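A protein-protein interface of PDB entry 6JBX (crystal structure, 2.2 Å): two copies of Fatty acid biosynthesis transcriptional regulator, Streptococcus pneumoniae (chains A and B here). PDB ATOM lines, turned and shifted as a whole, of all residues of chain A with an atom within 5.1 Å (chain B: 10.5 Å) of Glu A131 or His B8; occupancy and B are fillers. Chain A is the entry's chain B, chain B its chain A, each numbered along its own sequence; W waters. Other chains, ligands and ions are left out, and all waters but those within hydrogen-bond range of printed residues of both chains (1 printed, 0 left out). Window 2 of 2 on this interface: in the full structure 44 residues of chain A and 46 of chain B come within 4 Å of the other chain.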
ATOM      1  N   ILE A 126     -15.058  -1.608 -17.292  1.00  0.00           N
ATOM      2  CA  ILE A 126     -14.004  -1.933 -16.378  1.00  0.00           C
ATOM      3  C   ILE A 126     -14.494  -1.691 -14.937  1.00  0.00           C
ATOM      4  O   ILE A 126     -14.154  -2.448 -14.024  1.00  0.00           O
ATOM      5  CB  ILE A 126     -12.730  -1.144 -16.733  1.00  0.00           C
ATOM      6  CG1 ILE A 126     -12.073  -1.668 -18.017  1.00  0.00           C
ATOM      7  CG2 ILE A 126     -11.749  -1.119 -15.573  1.00  0.00           C
ATOM      8  CD1 ILE A 126     -10.899  -0.843 -18.518  1.00  0.00           C
ATOM      9  N   MET A 129     -16.087  -4.683 -13.074  1.00  0.00           N
ATOM     10  CA  MET A 129     -15.358  -5.958 -13.073  1.00  0.00           C
ATOM     11  C   MET A 129     -14.454  -6.041 -11.833  1.00  0.00           C
ATOM     12  O   MET A 129     -13.969  -5.015 -11.323  1.00  0.00           O
ATOM     13  CB  MET A 129     -14.477  -6.094 -14.323  1.00  0.00           C
ATOM     14  CG  MET A 129     -15.224  -6.551 -15.569  1.00  0.00           C
ATOM     15  SD  MET A 129     -14.269  -6.238 -17.101  1.00  0.00           S
ATOM     16  CE  MET A 129     -12.701  -6.996 -16.748  1.00  0.00           C
ATOM     17  N   SER A 130     -14.153  -7.274 -11.428  1.00  0.00           N
ATOM     18  CA  SER A 130     -13.305  -7.532 -10.261  1.00  0.00           C
ATOM     19  C   SER A 130     -11.860  -7.375 -10.697  1.00  0.00           C
ATOM     20  O   SER A 130     -11.567  -7.466 -11.889  1.00  0.00           O
ATOM     21  CB  SER A 130     -13.535  -8.919  -9.690  1.00  0.00           C
ATOM     22  OG  SER A 130     -12.812  -9.888 -10.443  1.00  0.00           O
ATOM     23  N   GLU A 131     -10.973  -7.165  -9.746  1.00  0.00           N
ATOM     24  CA  GLU A 131      -9.589  -6.989 -10.075  1.00  0.00           C
ATOM     25  C   GLU A 131      -9.065  -8.219 -10.837  1.00  0.00           C
ATOM     26  O   GLU A 131      -8.183  -8.105 -11.717  1.00  0.00           O
ATOM     27  CB  GLU A 131      -8.770  -6.715  -8.814  1.00  0.00           C
ATOM     28  CG  GLU A 131      -8.964  -5.302  -8.248  1.00  0.00           C
ATOM     29  CD  GLU A 131      -8.781  -4.145  -9.231  1.00  0.00           C
ATOM     30  OE1 GLU A 131      -9.771  -3.425  -9.492  1.00  0.00           O
ATOM     31  OE2 GLU A 131      -7.651  -3.964  -9.744  1.00  0.00           O
ATOM     32  N   GLU A 132      -9.563  -9.397 -10.488  1.00  0.00           N
ATOM     33  CA  GLU A 132      -9.054 -10.567 -11.113  1.00  0.00           C
ATOM     34  C   GLU A 132      -9.623 -10.682 -12.538  1.00  0.00           C
ATOM     35  O   GLU A 132      -8.894 -11.089 -13.440  1.00  0.00           O
ATOM     36  CB  GLU A 132      -9.368 -11.799 -10.273  1.00  0.00           C
ATOM     37  CG  GLU A 132      -8.883 -13.089 -10.902  1.00  0.00           C
ATOM     38  CD  GLU A 132      -7.372 -13.320 -10.967  1.00  0.00           C
ATOM     39  OE1 GLU A 132      -6.982 -14.495 -11.210  1.00  0.00           O
ATOM     40  OE2 GLU A 132      -6.579 -12.343 -10.796  1.00  0.00           O
ATOM     41  N   GLU A 133     -10.905 -10.388 -12.725  1.00  0.00           N
ATOM     42  CA  GLU A 133     -11.492 -10.287 -14.076  1.00  0.00           C
ATOM     43  C   GLU A 133     -10.674  -9.346 -14.976  1.00  0.00           C
ATOM     44  O   GLU A 133     -10.348  -9.710 -16.098  1.00  0.00           O
ATOM     45  CB  GLU A 133     -12.937  -9.816 -14.014  1.00  0.00           C
ATOM     46  CG  GLU A 133     -13.882 -10.944 -13.742  1.00  0.00           C
ATOM     47  CD  GLU A 133     -15.291 -10.486 -13.465  1.00  0.00           C
ATOM     48  OE1 GLU A 133     -15.470  -9.284 -13.233  1.00  0.00           O
ATOM     49  OE2 GLU A 133     -16.193 -11.346 -13.476  1.00  0.00           O
ATOM     50  N   ILE A 134     -10.297  -8.180 -14.470  1.00  0.00           N
ATOM     51  CA  ILE A 134      -9.611  -7.179 -15.290  1.00  0.00           C
ATOM     52  C   ILE A 134      -8.216  -7.697 -15.650  1.00  0.00           C
ATOM     53  O   ILE A 134      -7.740  -7.550 -16.808  1.00  0.00           O
ATOM     54  CB  ILE A 134      -9.564  -5.820 -14.565  1.00  0.00           C
ATOM     55  CG1 ILE A 134     -10.966  -5.286 -14.264  1.00  0.00           C
ATOM     56  CG2 ILE A 134      -8.757  -4.819 -15.370  1.00  0.00           C
ATOM     57  CD1 ILE A 134     -11.011  -4.079 -13.339  1.00  0.00           C
ATOM     58  N   ALA A 135      -7.533  -8.289 -14.684  1.00  0.00           N
ATOM     59  CA  ALA A 135      -6.220  -8.839 -14.984  1.00  0.00           C
ATOM     60  C   ALA A 135      -6.295  -9.867 -16.137  1.00  0.00           C
ATOM     61  O   ALA A 135      -5.449  -9.873 -17.060  1.00  0.00           O
ATOM     62  CB  ALA A 135      -5.639  -9.480 -13.747  1.00  0.00           C
ATOM     63  N   HIS B   7      -1.908  -3.852 -11.504  1.00  0.00           N
ATOM     64  CA  HIS B   7      -2.191  -2.528 -12.204  1.00  0.00           C
ATOM     65  C   HIS B   7      -2.964  -2.739 -13.519  1.00  0.00           C
ATOM     66  O   HIS B   7      -2.643  -3.638 -14.294  1.00  0.00           O
ATOM     67  CB  HIS B   7      -0.886  -1.767 -12.475  1.00  0.00           C
ATOM     68  CG  HIS B   7      -0.267  -1.175 -11.249  1.00  0.00           C
ATOM     69  ND1 HIS B   7      -0.922  -0.212 -10.473  1.00  0.00           N
ATOM     70  CD2 HIS B   7       0.937  -1.387 -10.670  1.00  0.00           C
ATOM     71  CE1 HIS B   7      -0.151   0.135  -9.462  1.00  0.00           C
ATOM     72  NE2 HIS B   7       1.001  -0.571  -9.570  1.00  0.00           N
ATOM     73  N   HIS B   8      -3.981  -1.917 -13.752  1.00  0.00           N
ATOM     74  CA  HIS B   8      -4.767  -1.973 -14.980  1.00  0.00           C
ATOM     75  C   HIS B   8      -3.870  -1.708 -16.190  1.00  0.00           C
ATOM     76  O   HIS B   8      -2.829  -1.074 -16.113  1.00  0.00           O
ATOM     77  CB  HIS B   8      -5.915  -0.955 -14.957  1.00  0.00           C
ATOM     78  CG  HIS B   8      -6.934  -1.208 -13.899  1.00  0.00           C
ATOM     79  ND1 HIS B   8      -7.983  -0.326 -13.664  1.00  0.00           N
ATOM     80  CD2 HIS B   8      -7.067  -2.220 -13.005  1.00  0.00           C
ATOM     81  CE1 HIS B   8      -8.729  -0.794 -12.677  1.00  0.00           C
ATOM     82  NE2 HIS B   8      -8.190  -1.960 -12.258  1.00  0.00           N
ATOM     83  N   MET B   9      -4.268  -2.225 -17.326  1.00  0.00           N
ATOM     84  CA  MET B   9      -3.642  -1.799 -18.582  1.00  0.00           C
ATOM     85  C   MET B   9      -3.968  -0.314 -18.823  1.00  0.00           C
ATOM     86  O   MET B   9      -5.067   0.151 -18.541  1.00  0.00           O
ATOM     87  CB  MET B   9      -4.205  -2.600 -19.758  1.00  0.00           C
ATOM     88  CG  MET B   9      -3.361  -3.753 -20.200  1.00  0.00           C
ATOM     89  SD  MET B   9      -4.163  -4.694 -21.540  1.00  0.00           S
ATOM     90  CE  MET B   9      -4.351  -3.390 -22.739  1.00  0.00           C
ATOM     91  N   ASP B  10      -3.027   0.387 -19.406  1.00  0.00           N
ATOM     92  CA  ASP B  10      -3.248   1.762 -19.874  1.00  0.00           C
ATOM     93  C   ASP B  10      -4.447   1.809 -20.832  1.00  0.00           C
ATOM     94  O   ASP B  10      -4.586   0.947 -21.722  1.00  0.00           O
ATOM     95  CB  ASP B  10      -1.989   2.259 -20.587  1.00  0.00           C
ATOM     96  CG  ASP B  10      -0.790   2.539 -19.686  1.00  0.00           C
ATOM     97  OD1 ASP B  10      -0.983   2.590 -18.448  1.00  0.00           O
ATOM     98  OD2 ASP B  10       0.324   2.729 -20.224  1.00  0.00           O
ATOM     99  N   TYR B  11      -5.305   2.791 -20.680  1.00  0.00           N
ATOM    100  CA  TYR B  11      -6.445   2.941 -21.598  1.00  0.00           C
ATOM    101  C   TYR B  11      -5.999   3.054 -23.064  1.00  0.00           C
ATOM    102  O   TYR B  11      -6.606   2.471 -23.937  1.00  0.00           O
ATOM    103  CB  TYR B  11      -7.348   4.127 -21.268  1.00  0.00           C
ATOM    104  CG  TYR B  11      -8.434   4.288 -22.315  1.00  0.00           C
ATOM    105  CD1 TYR B  11      -9.530   3.436 -22.343  1.00  0.00           C
ATOM    106  CD2 TYR B  11      -8.319   5.223 -23.336  1.00  0.00           C
ATOM    107  CE1 TYR B  11     -10.511   3.523 -23.322  1.00  0.00           C
ATOM    108  CE2 TYR B  11      -9.276   5.304 -24.347  1.00  0.00           C
ATOM    109  CZ  TYR B  11     -10.388   4.468 -24.332  1.00  0.00           C
ATOM    110  OH  TYR B  11     -11.346   4.546 -25.309  1.00  0.00           O
ATOM    111  N   GLN B  12      -4.925   3.758 -23.323  1.00  0.00           N
ATOM    112  CA  GLN B  12      -4.370   3.920 -24.675  1.00  0.00           C
ATOM    113  C   GLN B  12      -4.079   2.545 -25.313  1.00  0.00           C
ATOM    114  O   GLN B  12      -4.317   2.331 -26.537  1.00  0.00           O
ATOM    115  CB  GLN B  12      -3.117   4.804 -24.616  1.00  0.00           C
ATOM    116  CG  GLN B  12      -3.326   6.117 -23.809  1.00  0.00           C
ATOM    117  CD  GLN B  12      -2.828   6.182 -22.359  1.00  0.00           C
ATOM    118  OE1 GLN B  12      -3.463   5.640 -21.410  1.00  0.00           O
ATOM    119  NE2 GLN B  12      -1.708   6.899 -22.174  1.00  0.00           N
ATOM    120  N   ARG B  13      -3.584   1.603 -24.510  1.00  0.00           N
ATOM    121  CA  ARG B  13      -3.210   0.318 -25.049  1.00  0.00           C
ATOM    122  C   ARG B  13      -4.479  -0.497 -25.253  1.00  0.00           C
ATOM    123  O   ARG B  13      -4.611  -1.130 -26.282  1.00  0.00           O
ATOM    124  CB  ARG B  13      -2.220  -0.400 -24.137  1.00  0.00           C
ATOM    125  CG  ARG B  13      -1.822  -1.792 -24.609  1.00  0.00           C
ATOM    126  CD  ARG B  13      -0.571  -2.290 -23.916  1.00  0.00           C
ATOM    127  NE  ARG B  13       0.587  -1.639 -24.529  1.00  0.00           N
ATOM    128  CZ  ARG B  13       1.853  -1.994 -24.334  1.00  0.00           C
ATOM    129  NH1 ARG B  13       2.140  -3.033 -23.563  1.00  0.00           N
ATOM    130  NH2 ARG B  13       2.819  -1.310 -24.922  1.00  0.00           N
ATOM    131  N   ILE B  14      -5.418  -0.411 -24.324  1.00  0.00           N
ATOM    132  CA  ILE B  14      -6.715  -1.040 -24.460  1.00  0.00           C
ATOM    133  C   ILE B  14      -7.378  -0.578 -25.774  1.00  0.00           C
ATOM    134  O   ILE B  14      -7.872  -1.379 -26.559  1.00  0.00           O
ATOM    135  CB  ILE B  14      -7.607  -0.756 -23.237  1.00  0.00           C
ATOM    136  CG1 ILE B  14      -7.046  -1.379 -21.952  1.00  0.00           C
ATOM    137  CG2 ILE B  14      -9.007  -1.256 -23.479  1.00  0.00           C
ATOM    138  CD1 ILE B  14      -7.886  -1.152 -20.722  1.00  0.00           C
ATOM    139  N   GLU B 133      -7.388 -19.072 -14.172  1.00  0.00           N
ATOM    140  CA  GLU B 133      -7.493 -17.806 -14.938  1.00  0.00           C
ATOM    141  C   GLU B 133      -8.507 -18.009 -16.072  1.00  0.00           C
ATOM    142  O   GLU B 133      -9.373 -17.209 -16.246  1.00  0.00           O
ATOM    143  CB  GLU B 133      -6.111 -17.405 -15.455  1.00  0.00           C
ATOM    144  CG  GLU B 133      -5.202 -16.753 -14.418  1.00  0.00           C
ATOM    145  CD  GLU B 133      -3.770 -16.543 -14.914  1.00  0.00           C
ATOM    146  OE1 GLU B 133      -3.225 -17.448 -15.554  1.00  0.00           O
ATOM    147  OE2 GLU B 133      -3.200 -15.461 -14.672  1.00  0.00           O
ATOM    148  N   VAL B 136     -11.871 -17.751 -14.655  1.00  0.00           N
ATOM    149  CA  VAL B 136     -12.204 -16.360 -14.407  1.00  0.00           C
ATOM    150  C   VAL B 136     -12.573 -15.688 -15.744  1.00  0.00           C
ATOM    151  O   VAL B 136     -13.574 -14.953 -15.846  1.00  0.00           O
ATOM    152  CB  VAL B 136     -11.050 -15.626 -13.708  1.00  0.00           C
ATOM    153  CG1 VAL B 136     -11.299 -14.122 -13.677  1.00  0.00           C
ATOM    154  CG2 VAL B 136     -10.829 -16.164 -12.301  1.00  0.00           C
ATOM    155  N   MET B 137     -11.792 -15.990 -16.775  1.00  0.00           N
ATOM    156  CA  MET B 137     -12.017 -15.418 -18.119  1.00  0.00           C
ATOM    157  C   MET B 137     -13.407 -15.810 -18.631  1.00  0.00           C
ATOM    158  O   MET B 137     -14.109 -15.009 -19.235  1.00  0.00           O
ATOM    159  CB  MET B 137     -10.950 -15.893 -19.113  1.00  0.00           C
ATOM    160  CG  MET B 137     -10.975 -15.092 -20.401  1.00  0.00           C
ATOM    161  SD  MET B 137     -10.224 -15.942 -21.776  1.00  0.00           S
ATOM    162  CE  MET B 137     -11.239 -17.416 -21.906  1.00  0.00           C
ATOM    163  N   GLY B 140     -15.755 -13.536 -16.845  1.00  0.00           N
ATOM    164  CA  GLY B 140     -15.566 -12.203 -17.428  1.00  0.00           C
ATOM    165  C   GLY B 140     -16.336 -12.054 -18.734  1.00  0.00           C
ATOM    166  O   GLY B 140     -17.033 -11.055 -18.924  1.00  0.00           O
ATOM    167  N   ASN B 143     -20.143 -11.925 -18.194  1.00  0.00           N
ATOM    168  CA  ASN B 143     -20.485 -10.621 -17.615  1.00  0.00           C
ATOM    169  C   ASN B 143     -20.407  -9.515 -18.689  1.00  0.00           C
ATOM    170  O   ASN B 143     -21.279  -8.655 -18.759  1.00  0.00           O
ATOM    171  CB  ASN B 143     -19.593 -10.309 -16.402  1.00  0.00           C
ATOM    172  CG  ASN B 143     -19.798 -11.268 -15.229  1.00  0.00           C
ATOM    173  OD1 ASN B 143     -20.682 -12.126 -15.245  1.00  0.00           O
ATOM    174  ND2 ASN B 143     -18.988 -11.130 -14.185  1.00  0.00           N
HETATM  175  O   HOH W   1      -5.768  -5.209 -17.035  1.00  0.00           O
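Ile A126 touches Ile B14 (CD1 to CD1, 3.7 Å).
Val B136 touches Glu A132 (CG1 to CG, 3.8 Å).
CA of Glu A133 touches CG1 of Val B136, 3.9 Å away.
Ile A134 touches His B8 (CD1 to NE2, 3.7 Å).
The backbone NH (N) of Glu A132 sits close to the side-chain hydroxyl (OG) of Ser A130 (3.3 Å).
N of Ser A130 sits at hydrogen-bond distance from OE1 of Glu A133 (3.0 Å).
The side-chain carboxylate (OE2) of Glu A133 is in hydrogen-bond range of the side-chain amide nitrogen (ND2) of Asn B143, 2.9 Å away.
The side-chain carboxylate (OE2) of Glu A131 sits at hydrogen-bond distance from a ring nitrogen (NE2) of His B8 (3.3 Å).
Met A129 touches none of the printed residues of chain B.
No residue of chain B comes within 4 Å of Ser A130.
Glu A131 touches just one residue of chain B: His B8 (3.3 Å).
Printed residues of chain B within 4 Å of Glu A132: Val B136.
Of chain B, only His B8 comes within 4 Å of Ile A134.
Ala A135 touches none of the printed residues of chain B.
Of chain A, only Glu A131 (3.3 Å) and Ile A134 (3.7 Å) come within 4 Å of His B8.
Printed residues of chain A within 4 Å of Val B136: Glu A132 (3.8 Å) and Glu A133 (3.9 Å).
The nearest residue of chain B that does not touch Glu A131 is His B7 (6.0 Å).
Of the 8 printed residues of chain A, 5 touch a printed residue of chain B.
Hydrophobic or aromatic side chains of chain A that line the printed part of chain B: Ile A126 and Ile A134.
Among the printed residues, 6 pairs touch across the chains.
Among the printed residues, no Asp or Glu carboxylate lies within 4 Å of a Lys or Arg side-chain nitrogen of the other chain.
Water W1 bridges the backbone carbonyl oxygen (O) of Ile A134 and the backbone NH (N) of Met B9.
Position printed for both chains: 133.
Of the 6 pairs that touch across the chains among the printed residues, none has its exchanged pair printed and touching as well.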
